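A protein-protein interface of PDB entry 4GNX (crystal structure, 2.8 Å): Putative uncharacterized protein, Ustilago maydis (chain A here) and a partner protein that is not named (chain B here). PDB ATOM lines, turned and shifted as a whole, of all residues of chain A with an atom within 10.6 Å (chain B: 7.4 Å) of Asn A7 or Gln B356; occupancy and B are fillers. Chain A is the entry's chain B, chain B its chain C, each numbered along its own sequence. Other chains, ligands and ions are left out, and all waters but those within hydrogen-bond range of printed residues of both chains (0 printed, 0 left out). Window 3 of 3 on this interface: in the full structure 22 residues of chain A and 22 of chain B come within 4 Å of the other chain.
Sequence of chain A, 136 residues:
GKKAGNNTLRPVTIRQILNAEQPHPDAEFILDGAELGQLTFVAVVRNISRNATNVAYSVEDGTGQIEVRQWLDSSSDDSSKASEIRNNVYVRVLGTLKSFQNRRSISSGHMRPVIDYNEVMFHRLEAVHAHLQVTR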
ATOM      1  N   ASN A   7      33.797  13.400  -0.174  1.00  0.00           N
ATOM      2  CA  ASN A   7      32.650  13.924   0.638  1.00  0.00           C
ATOM      3  C   ASN A   7      31.344  13.972  -0.171  1.00  0.00           C
ATOM      4  O   ASN A   7      31.263  14.632  -1.195  1.00  0.00           O
ATOM      5  CB  ASN A   7      33.005  15.296   1.184  1.00  0.00           C
ATOM      6  CG  ASN A   7      32.055  15.756   2.252  1.00  0.00           C
ATOM      7  OD1 ASN A   7      30.929  15.273   2.350  1.00  0.00           O
ATOM      8  ND2 ASN A   7      32.504  16.716   3.060  1.00  0.00           N
ATOM      9  N   THR A   8      30.316  13.276   0.292  1.00  0.00           N
ATOM     10  CA  THR A   8      29.267  12.829  -0.604  1.00  0.00           C
ATOM     11  C   THR A   8      27.890  12.940  -0.001  1.00  0.00           C
ATOM     12  O   THR A   8      27.758  13.197   1.191  1.00  0.00           O
ATOM     13  CB  THR A   8      29.456  11.337  -0.968  1.00  0.00           C
ATOM     14  OG1 THR A   8      29.377  10.528   0.221  1.00  0.00           O
ATOM     15  CG2 THR A   8      30.793  11.094  -1.701  1.00  0.00           C
ATOM     16  N   LEU A   9      26.872  12.713  -0.836  1.00  0.00           N
ATOM     17  CA  LEU A   9      25.481  12.742  -0.440  1.00  0.00           C
ATOM     18  C   LEU A   9      24.822  11.442  -0.875  1.00  0.00           C
ATOM     19  O   LEU A   9      24.405  11.285  -2.023  1.00  0.00           O
ATOM     20  CB  LEU A   9      24.753  13.940  -1.061  1.00  0.00           C
ATOM     21  CG  LEU A   9      23.232  13.942  -0.843  1.00  0.00           C
ATOM     22  CD1 LEU A   9      22.919  14.216   0.618  1.00  0.00           C
ATOM     23  CD2 LEU A   9      22.506  14.906  -1.778  1.00  0.00           C
ATOM     24  N   ARG A  10      24.691  10.526   0.074  1.00  0.00           N
ATOM     25  CA  ARG A  10      24.312   9.153  -0.225  1.00  0.00           C
ATOM     26  C   ARG A  10      22.829   8.854  -0.082  1.00  0.00           C
ATOM     27  O   ARG A  10      22.240   9.052   0.976  1.00  0.00           O
ATOM     28  CB  ARG A  10      25.155   8.186   0.605  1.00  0.00           C
ATOM     29  CG  ARG A  10      26.639   8.412   0.383  1.00  0.00           C
ATOM     30  CD  ARG A  10      27.493   7.455   1.199  1.00  0.00           C
ATOM     31  NE  ARG A  10      26.990   6.084   1.133  1.00  0.00           N
ATOM     32  CZ  ARG A  10      27.561   5.041   1.724  1.00  0.00           C
ATOM     33  NH1 ARG A  10      28.663   5.183   2.444  1.00  0.00           N
ATOM     34  NH2 ARG A  10      26.995   3.848   1.600  1.00  0.00           N
ATOM     35  N   GLU A  28      33.270   8.117  12.745  1.00  0.00           N
ATOM     36  CA  GLU A  28      32.460   8.220  11.548  1.00  0.00           C
ATOM     37  C   GLU A  28      31.712   6.906  11.373  1.00  0.00           C
ATOM     38  O   GLU A  28      32.206   5.853  11.773  1.00  0.00           O
ATOM     39  CB  GLU A  28      33.360   8.471  10.333  1.00  0.00           C
ATOM     40  CG  GLU A  28      34.103   9.805  10.358  1.00  0.00           C
ATOM     41  CD  GLU A  28      35.384   9.793   9.522  1.00  0.00           C
ATOM     42  OE1 GLU A  28      35.315   9.475   8.307  1.00  0.00           O
ATOM     43  OE2 GLU A  28      36.467  10.106  10.077  1.00  0.00           O
ATOM     44  N   ALA A  34      32.182   2.352   3.186  1.00  0.00           N
ATOM     45  CA  ALA A  34      32.373   3.740   2.806  1.00  0.00           C
ATOM     46  C   ALA A  34      31.839   4.652   3.884  1.00  0.00           C
ATOM     47  O   ALA A  34      30.835   4.341   4.529  1.00  0.00           O
ATOM     48  CB  ALA A  34      31.709   4.026   1.476  1.00  0.00           C
ATOM     49  N   GLU A  35      32.532   5.767   4.081  1.00  0.00           N
ATOM     50  CA  GLU A  35      32.132   6.782   5.024  1.00  0.00           C
ATOM     51  C   GLU A  35      30.695   7.209   4.734  1.00  0.00           C
ATOM     52  O   GLU A  35      30.322   7.403   3.575  1.00  0.00           O
ATOM     53  CB  GLU A  35      33.074   7.971   4.892  1.00  0.00           C
ATOM     54  CG  GLU A  35      33.313   8.761   6.176  1.00  0.00           C
ATOM     55  CD  GLU A  35      32.633  10.131   6.206  1.00  0.00           C
ATOM     56  OE1 GLU A  35      31.601  10.331   5.508  1.00  0.00           O
ATOM     57  OE2 GLU A  35      33.139  11.017   6.946  1.00  0.00           O
ATOM     58  N   LEU A  36      29.895   7.321   5.794  1.00  0.00           N
ATOM     59  CA  LEU A  36      28.497   7.738   5.703  1.00  0.00           C
ATOM     60  C   LEU A  36      28.303   9.064   6.415  1.00  0.00           C
ATOM     61  O   LEU A  36      28.020   9.104   7.615  1.00  0.00           O
ATOM     62  CB  LEU A  36      27.582   6.698   6.338  1.00  0.00           C
ATOM     63  CG  LEU A  36      26.067   6.928   6.260  1.00  0.00           C
ATOM     64  CD1 LEU A  36      25.542   7.011   4.823  1.00  0.00           C
ATOM     65  CD2 LEU A  36      25.364   5.812   7.015  1.00  0.00           C
ATOM     66  N   GLY A  37      28.468  10.148   5.663  1.00  0.00           N
ATOM     67  CA  GLY A  37      28.353  11.492   6.201  1.00  0.00           C
ATOM     68  C   GLY A  37      26.962  12.031   5.943  1.00  0.00           C
ATOM     69  O   GLY A  37      25.995  11.629   6.601  1.00  0.00           O
ATOM     70  N   GLN A  38      26.865  12.943   4.982  1.00  0.00           N
ATOM     71  CA  GLN A  38      25.584  13.455   4.561  1.00  0.00           C
ATOM     72  C   GLN A  38      24.850  12.373   3.819  1.00  0.00           C
ATOM     73  O   GLN A  38      25.471  11.572   3.128  1.00  0.00           O
ATOM     74  CB  GLN A  38      25.764  14.654   3.653  1.00  0.00           C
ATOM     75  CG  GLN A  38      25.779  15.978   4.380  1.00  0.00           C
ATOM     76  CD  GLN A  38      25.317  17.129   3.494  1.00  0.00           C
ATOM     77  OE1 GLN A  38      24.332  17.799   3.812  1.00  0.00           O
ATOM     78  NE2 GLN A  38      26.026  17.367   2.381  1.00  0.00           N
ATOM     79  N   LEU A  39      23.529  12.362   3.953  1.00  0.00           N
ATOM     80  CA  LEU A  39      22.697  11.345   3.337  1.00  0.00           C
ATOM     81  C   LEU A  39      21.312  11.903   3.051  1.00  0.00           C
ATOM     82  O   LEU A  39      20.917  12.922   3.611  1.00  0.00           O
ATOM     83  CB  LEU A  39      22.577  10.145   4.269  1.00  0.00           C
ATOM     84  CG  LEU A  39      21.968  10.353   5.673  1.00  0.00           C
ATOM     85  CD1 LEU A  39      20.452  10.174   5.670  1.00  0.00           C
ATOM     86  CD2 LEU A  39      22.577   9.378   6.664  1.00  0.00           C
ATOM     87  N   LEU A  94      17.130  15.634   3.968  1.00  0.00           N
ATOM     88  CA  LEU A  94      18.568  15.783   3.806  1.00  0.00           C
ATOM     89  C   LEU A  94      19.180  15.989   5.195  1.00  0.00           C
ATOM     90  O   LEU A  94      18.668  16.798   5.978  1.00  0.00           O
ATOM     91  CB  LEU A  94      18.854  16.972   2.897  1.00  0.00           C
ATOM     92  CG  LEU A  94      20.249  16.981   2.291  1.00  0.00           C
ATOM     93  CD1 LEU A  94      20.242  17.509   0.869  1.00  0.00           C
ATOM     94  CD2 LEU A  94      21.156  17.823   3.153  1.00  0.00           C
ATOM     95  N   GLY A  95      20.257  15.285   5.532  1.00  0.00           N
ATOM     96  CA  GLY A  95      20.757  15.368   6.916  1.00  0.00           C
ATOM     97  C   GLY A  95      22.091  14.713   7.179  1.00  0.00           C
ATOM     98  O   GLY A  95      22.703  14.213   6.268  1.00  0.00           O
ATOM     99  N   THR A  96      22.550  14.742   8.424  1.00  0.00           N
ATOM    100  CA  THR A  96      23.750  14.011   8.819  1.00  0.00           C
ATOM    101  C   THR A  96      23.351  12.955   9.849  1.00  0.00           C
ATOM    102  O   THR A  96      22.511  13.217  10.724  1.00  0.00           O
ATOM    103  CB  THR A  96      24.827  14.936   9.434  1.00  0.00           C
ATOM    104  OG1 THR A  96      24.872  16.176   8.727  1.00  0.00           O
ATOM    105  CG2 THR A  96      26.199  14.308   9.339  1.00  0.00           C
ATOM    106  N   ILE B 275      29.723  13.436 -10.515  1.00  0.00           N
ATOM    107  CA  ILE B 275      30.677  14.424 -10.039  1.00  0.00           C
ATOM    108  C   ILE B 275      32.100  13.832  -9.926  1.00  0.00           C
ATOM    109  O   ILE B 275      33.113  14.504 -10.232  1.00  0.00           O
ATOM    110  CB  ILE B 275      30.202  15.016  -8.701  1.00  0.00           C
ATOM    111  CG1 ILE B 275      28.916  15.822  -8.913  1.00  0.00           C
ATOM    112  CG2 ILE B 275      31.301  15.837  -8.041  1.00  0.00           C
ATOM    113  CD1 ILE B 275      28.147  16.117  -7.644  1.00  0.00           C
ATOM    114  N   VAL B 276      32.191  12.570  -9.512  1.00  0.00           N
ATOM    115  CA  VAL B 276      33.498  11.969  -9.420  1.00  0.00           C
ATOM    116  C   VAL B 276      34.102  11.832 -10.819  1.00  0.00           C
ATOM    117  O   VAL B 276      35.294  12.096 -11.003  1.00  0.00           O
ATOM    118  CB  VAL B 276      33.499  10.642  -8.652  1.00  0.00           C
ATOM    119  CG1 VAL B 276      32.769   9.549  -9.416  1.00  0.00           C
ATOM    120  CG2 VAL B 276      34.928  10.223  -8.364  1.00  0.00           C
ATOM    121  N   LYS B 279      35.477  15.269 -12.202  1.00  0.00           N
ATOM    122  CA  LYS B 279      36.798  15.569 -11.624  1.00  0.00           C
ATOM    123  C   LYS B 279      37.904  14.583 -12.029  1.00  0.00           C
ATOM    124  O   LYS B 279      39.000  15.009 -12.372  1.00  0.00           O
ATOM    125  CB  LYS B 279      36.709  15.663 -10.109  1.00  0.00           C
ATOM    126  CG  LYS B 279      35.847  16.806  -9.602  1.00  0.00           C
ATOM    127  CD  LYS B 279      35.122  16.372  -8.342  1.00  0.00           C
ATOM    128  CE  LYS B 279      34.627  17.542  -7.513  1.00  0.00           C
ATOM    129  NZ  LYS B 279      35.756  18.296  -6.915  1.00  0.00           N
ATOM    130  N   VAL B 299      22.618  21.552  -2.475  1.00  0.00           N
ATOM    131  CA  VAL B 299      22.903  21.454  -1.047  1.00  0.00           C
ATOM    132  C   VAL B 299      23.145  22.830  -0.395  1.00  0.00           C
ATOM    133  O   VAL B 299      22.887  22.999   0.796  1.00  0.00           O
ATOM    134  CB  VAL B 299      24.117  20.530  -0.845  1.00  0.00           C
ATOM    135  CG1 VAL B 299      24.952  20.937   0.345  1.00  0.00           C
ATOM    136  CG2 VAL B 299      23.667  19.092  -0.731  1.00  0.00           C
ATOM    137  N   ASN B 349      26.601  24.978  -4.376  1.00  0.00           N
ATOM    138  CA  ASN B 349      27.225  23.682  -4.122  1.00  0.00           C
ATOM    139  C   ASN B 349      26.247  22.503  -4.288  1.00  0.00           C
ATOM    140  O   ASN B 349      25.241  22.395  -3.578  1.00  0.00           O
ATOM    141  CB  ASN B 349      27.849  23.664  -2.721  1.00  0.00           C
ATOM    142  CG  ASN B 349      28.743  22.451  -2.481  1.00  0.00           C
ATOM    143  OD1 ASN B 349      28.462  21.641  -1.618  1.00  0.00           O
ATOM    144  ND2 ASN B 349      29.828  22.332  -3.239  1.00  0.00           N
ATOM    145  N   VAL B 350      26.553  21.616  -5.230  1.00  0.00           N
ATOM    146  CA  VAL B 350      25.682  20.490  -5.544  1.00  0.00           C
ATOM    147  C   VAL B 350      26.390  19.190  -5.245  1.00  0.00           C
ATOM    148  O   VAL B 350      27.612  19.100  -5.380  1.00  0.00           O
ATOM    149  CB  VAL B 350      25.193  20.498  -7.019  1.00  0.00           C
ATOM    150  CG1 VAL B 350      24.539  21.833  -7.360  1.00  0.00           C
ATOM    151  CG2 VAL B 350      26.314  20.162  -7.997  1.00  0.00           C
ATOM    152  N   ALA B 351      25.618  18.185  -4.834  1.00  0.00           N
ATOM    153  CA  ALA B 351      26.173  16.883  -4.458  1.00  0.00           C
ATOM    154  C   ALA B 351      25.397  15.738  -5.069  1.00  0.00           C
ATOM    155  O   ALA B 351      24.230  15.881  -5.400  1.00  0.00           O
ATOM    156  CB  ALA B 351      26.194  16.737  -2.953  1.00  0.00           C
ATOM    157  N   ASP B 352      26.077  14.616  -5.249  1.00  0.00           N
ATOM    158  CA  ASP B 352      25.438  13.337  -5.537  1.00  0.00           C
ATOM    159  C   ASP B 352      26.118  12.288  -4.664  1.00  0.00           C
ATOM    160  O   ASP B 352      26.748  12.647  -3.661  1.00  0.00           O
ATOM    161  CB  ASP B 352      25.491  12.997  -7.029  1.00  0.00           C
ATOM    162  CG  ASP B 352      26.931  12.774  -7.575  1.00  0.00           C
ATOM    163  OD1 ASP B 352      27.929  12.789  -6.795  1.00  0.00           O
ATOM    164  OD2 ASP B 352      27.046  12.572  -8.828  1.00  0.00           O
ATOM    165  N   ALA B 353      26.025  11.009  -5.032  1.00  0.00           N
ATOM    166  CA  ALA B 353      26.620   9.948  -4.201  1.00  0.00           C
ATOM    167  C   ALA B 353      28.123   9.778  -4.398  1.00  0.00           C
ATOM    168  O   ALA B 353      28.769   9.031  -3.653  1.00  0.00           O
ATOM    169  CB  ALA B 353      25.907   8.632  -4.397  1.00  0.00           C
ATOM    170  N   THR B 354      28.687  10.476  -5.380  1.00  0.00           N
ATOM    171  CA  THR B 354      30.104  10.334  -5.722  1.00  0.00           C
ATOM    172  C   THR B 354      30.936  11.529  -5.268  1.00  0.00           C
ATOM    173  O   THR B 354      32.157  11.505  -5.334  1.00  0.00           O
ATOM    174  CB  THR B 354      30.281  10.133  -7.238  1.00  0.00           C
ATOM    175  OG1 THR B 354      29.744  11.261  -7.952  1.00  0.00           O
ATOM    176  CG2 THR B 354      29.570   8.843  -7.704  1.00  0.00           C
ATOM    177  N   GLY B 355      30.275  12.580  -4.807  1.00  0.00           N
ATOM    178  CA  GLY B 355      30.976  13.805  -4.437  1.00  0.00           C
ATOM    179  C   GLY B 355      30.162  15.087  -4.448  1.00  0.00           C
ATOM    180  O   GLY B 355      28.932  15.092  -4.623  1.00  0.00           O
ATOM    181  N   GLN B 356      30.854  16.191  -4.255  1.00  0.00           N
ATOM    182  CA  GLN B 356      30.206  17.481  -4.163  1.00  0.00           C
ATOM    183  C   GLN B 356      30.943  18.469  -5.094  1.00  0.00           C
ATOM    184  O   GLN B 356      32.146  18.373  -5.297  1.00  0.00           O
ATOM    185  CB  GLN B 356      30.127  17.885  -2.679  1.00  0.00           C
ATOM    186  CG  GLN B 356      30.690  19.242  -2.288  1.00  0.00           C
ATOM    187  CD  GLN B 356      32.196  19.313  -2.398  1.00  0.00           C
ATOM    188  OE1 GLN B 356      32.913  18.501  -1.801  1.00  0.00           O
ATOM    189  NE2 GLN B 356      32.688  20.288  -3.171  1.00  0.00           N
ATOM    190  N   MET B 357      30.220  19.396  -5.689  1.00  0.00           N
ATOM    191  CA  MET B 357      30.831  20.269  -6.676  1.00  0.00           C
ATOM    192  C   MET B 357      30.173  21.641  -6.754  1.00  0.00           C
ATOM    193  O   MET B 357      28.952  21.762  -6.659  1.00  0.00           O
ATOM    194  CB  MET B 357      30.775  19.576  -8.035  1.00  0.00           C
ATOM    195  CG  MET B 357      30.748  20.483  -9.251  1.00  0.00           C
ATOM    196  SD  MET B 357      29.955  19.631 -10.621  1.00  0.00           S
ATOM    197  CE  MET B 357      31.285  18.522 -11.084  1.00  0.00           C
ATOM    198  N   TRP B 358      30.997  22.660  -6.979  1.00  0.00           N
ATOM    199  CA  TRP B 358      30.517  24.037  -7.130  1.00  0.00           C
ATOM    200  C   TRP B 358      30.158  24.415  -8.525  1.00  0.00           C
ATOM    201  O   TRP B 358      30.949  24.200  -9.450  1.00  0.00           O
ATOM    202  CB  TRP B 358      31.574  24.974  -6.638  1.00  0.00           C
ATOM    203  CG  TRP B 358      31.641  25.000  -5.132  1.00  0.00           C
ATOM    204  CD1 TRP B 358      32.517  24.315  -4.314  1.00  0.00           C
ATOM    205  CD2 TRP B 358      30.779  25.753  -4.221  1.00  0.00           C
ATOM    206  NE1 TRP B 358      32.266  24.589  -3.005  1.00  0.00           N
ATOM    207  CE2 TRP B 358      31.245  25.444  -2.875  1.00  0.00           C
ATOM    208  CE3 TRP B 358      29.720  26.640  -4.386  1.00  0.00           C
ATOM    209  CZ2 TRP B 358      30.667  26.005  -1.745  1.00  0.00           C
ATOM    210  CZ3 TRP B 358      29.134  27.193  -3.241  1.00  0.00           C
ATOM    211  CH2 TRP B 358      29.597  26.882  -1.950  1.00  0.00           C
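The side-chain carboxylate (OD2) of Asp B352 is in hydrogen-bond range of the backbone NH (N) of Ile B275 (3.3 Å).
N of Ile B275 sits at hydrogen-bond distance from OG1 of Thr B354 (3.4 Å).
The backbone NH (N) of Val B276 is in hydrogen-bond range of the side-chain hydroxyl (OG1) of Thr B354 (3.2 Å).
OD1 of Asp B352 lies within hydrogen-bond range of OG1 of Thr B354, 2.6 Å away.
The side-chain carboxylate (OD1) of Asp B352 is in hydrogen-bond range of the backbone NH (N) of Gly B355 (3.1 Å).
N of Gln B356 is in hydrogen-bond range of O of Asn A7.
The backbone carbonyl oxygen of Asp B352 lies within hydrogen-bond range of the backbone NH of Leu A9 (2.8 Å).
O of Leu A9 lies close to N of Ala B353, 3.4 Å away.
Along chain B the printed residues that touch a printed residue of chain A span positions 351 to 356.
Of the 14 printed residues of chain A, 3 touch a printed residue of chain B.
Among the printed residues, no Asp or Glu carboxylate lies within 4 Å of a Lys or Arg side-chain nitrogen of the other chain.
Among the printed residues, pairs that only touch across the chains: Asn A7 with Gly B355 (3.4 Å), Thr A8 with Gly B355 (3.5 Å), Thr A8 with Ala B353 (3.5 Å), Thr A8 with Thr B354 (3.6 Å), Leu A9 with Ala B351 (3.7 Å) and Thr A8 with Asp B352 (3.8 Å).
Of chain B, only Gly B355 and Gln B356 come within 4 Å of Asn A7.
Printed residues of chain A within 4 Å of Gln B356: Asn A7 (3.5 Å).
Of chain A, only Leu A9 comes within 4 Å of Ala B351.
No residue of chain A comes within 4 Å of Met B357.
Printed residues of chain B within 4 Å of Leu A9: Ala B351, Asp B352 and Ala B353.
Of the printed residues of chain B, Thr A8 touches Asp B352, Ala B353, Thr B354 and Gly B355.
Of the printed residues of chain A, Ala B353 touches Thr A8 (3.5 Å) and Leu A9 (3.4 Å).
Of the printed residues of chain A, Thr B354 touches Thr A8.
Printed residues of chain A within 4 Å of Asp B352: Thr A8 and Leu A9.
Val B299 touches none of the printed residues of chain A.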
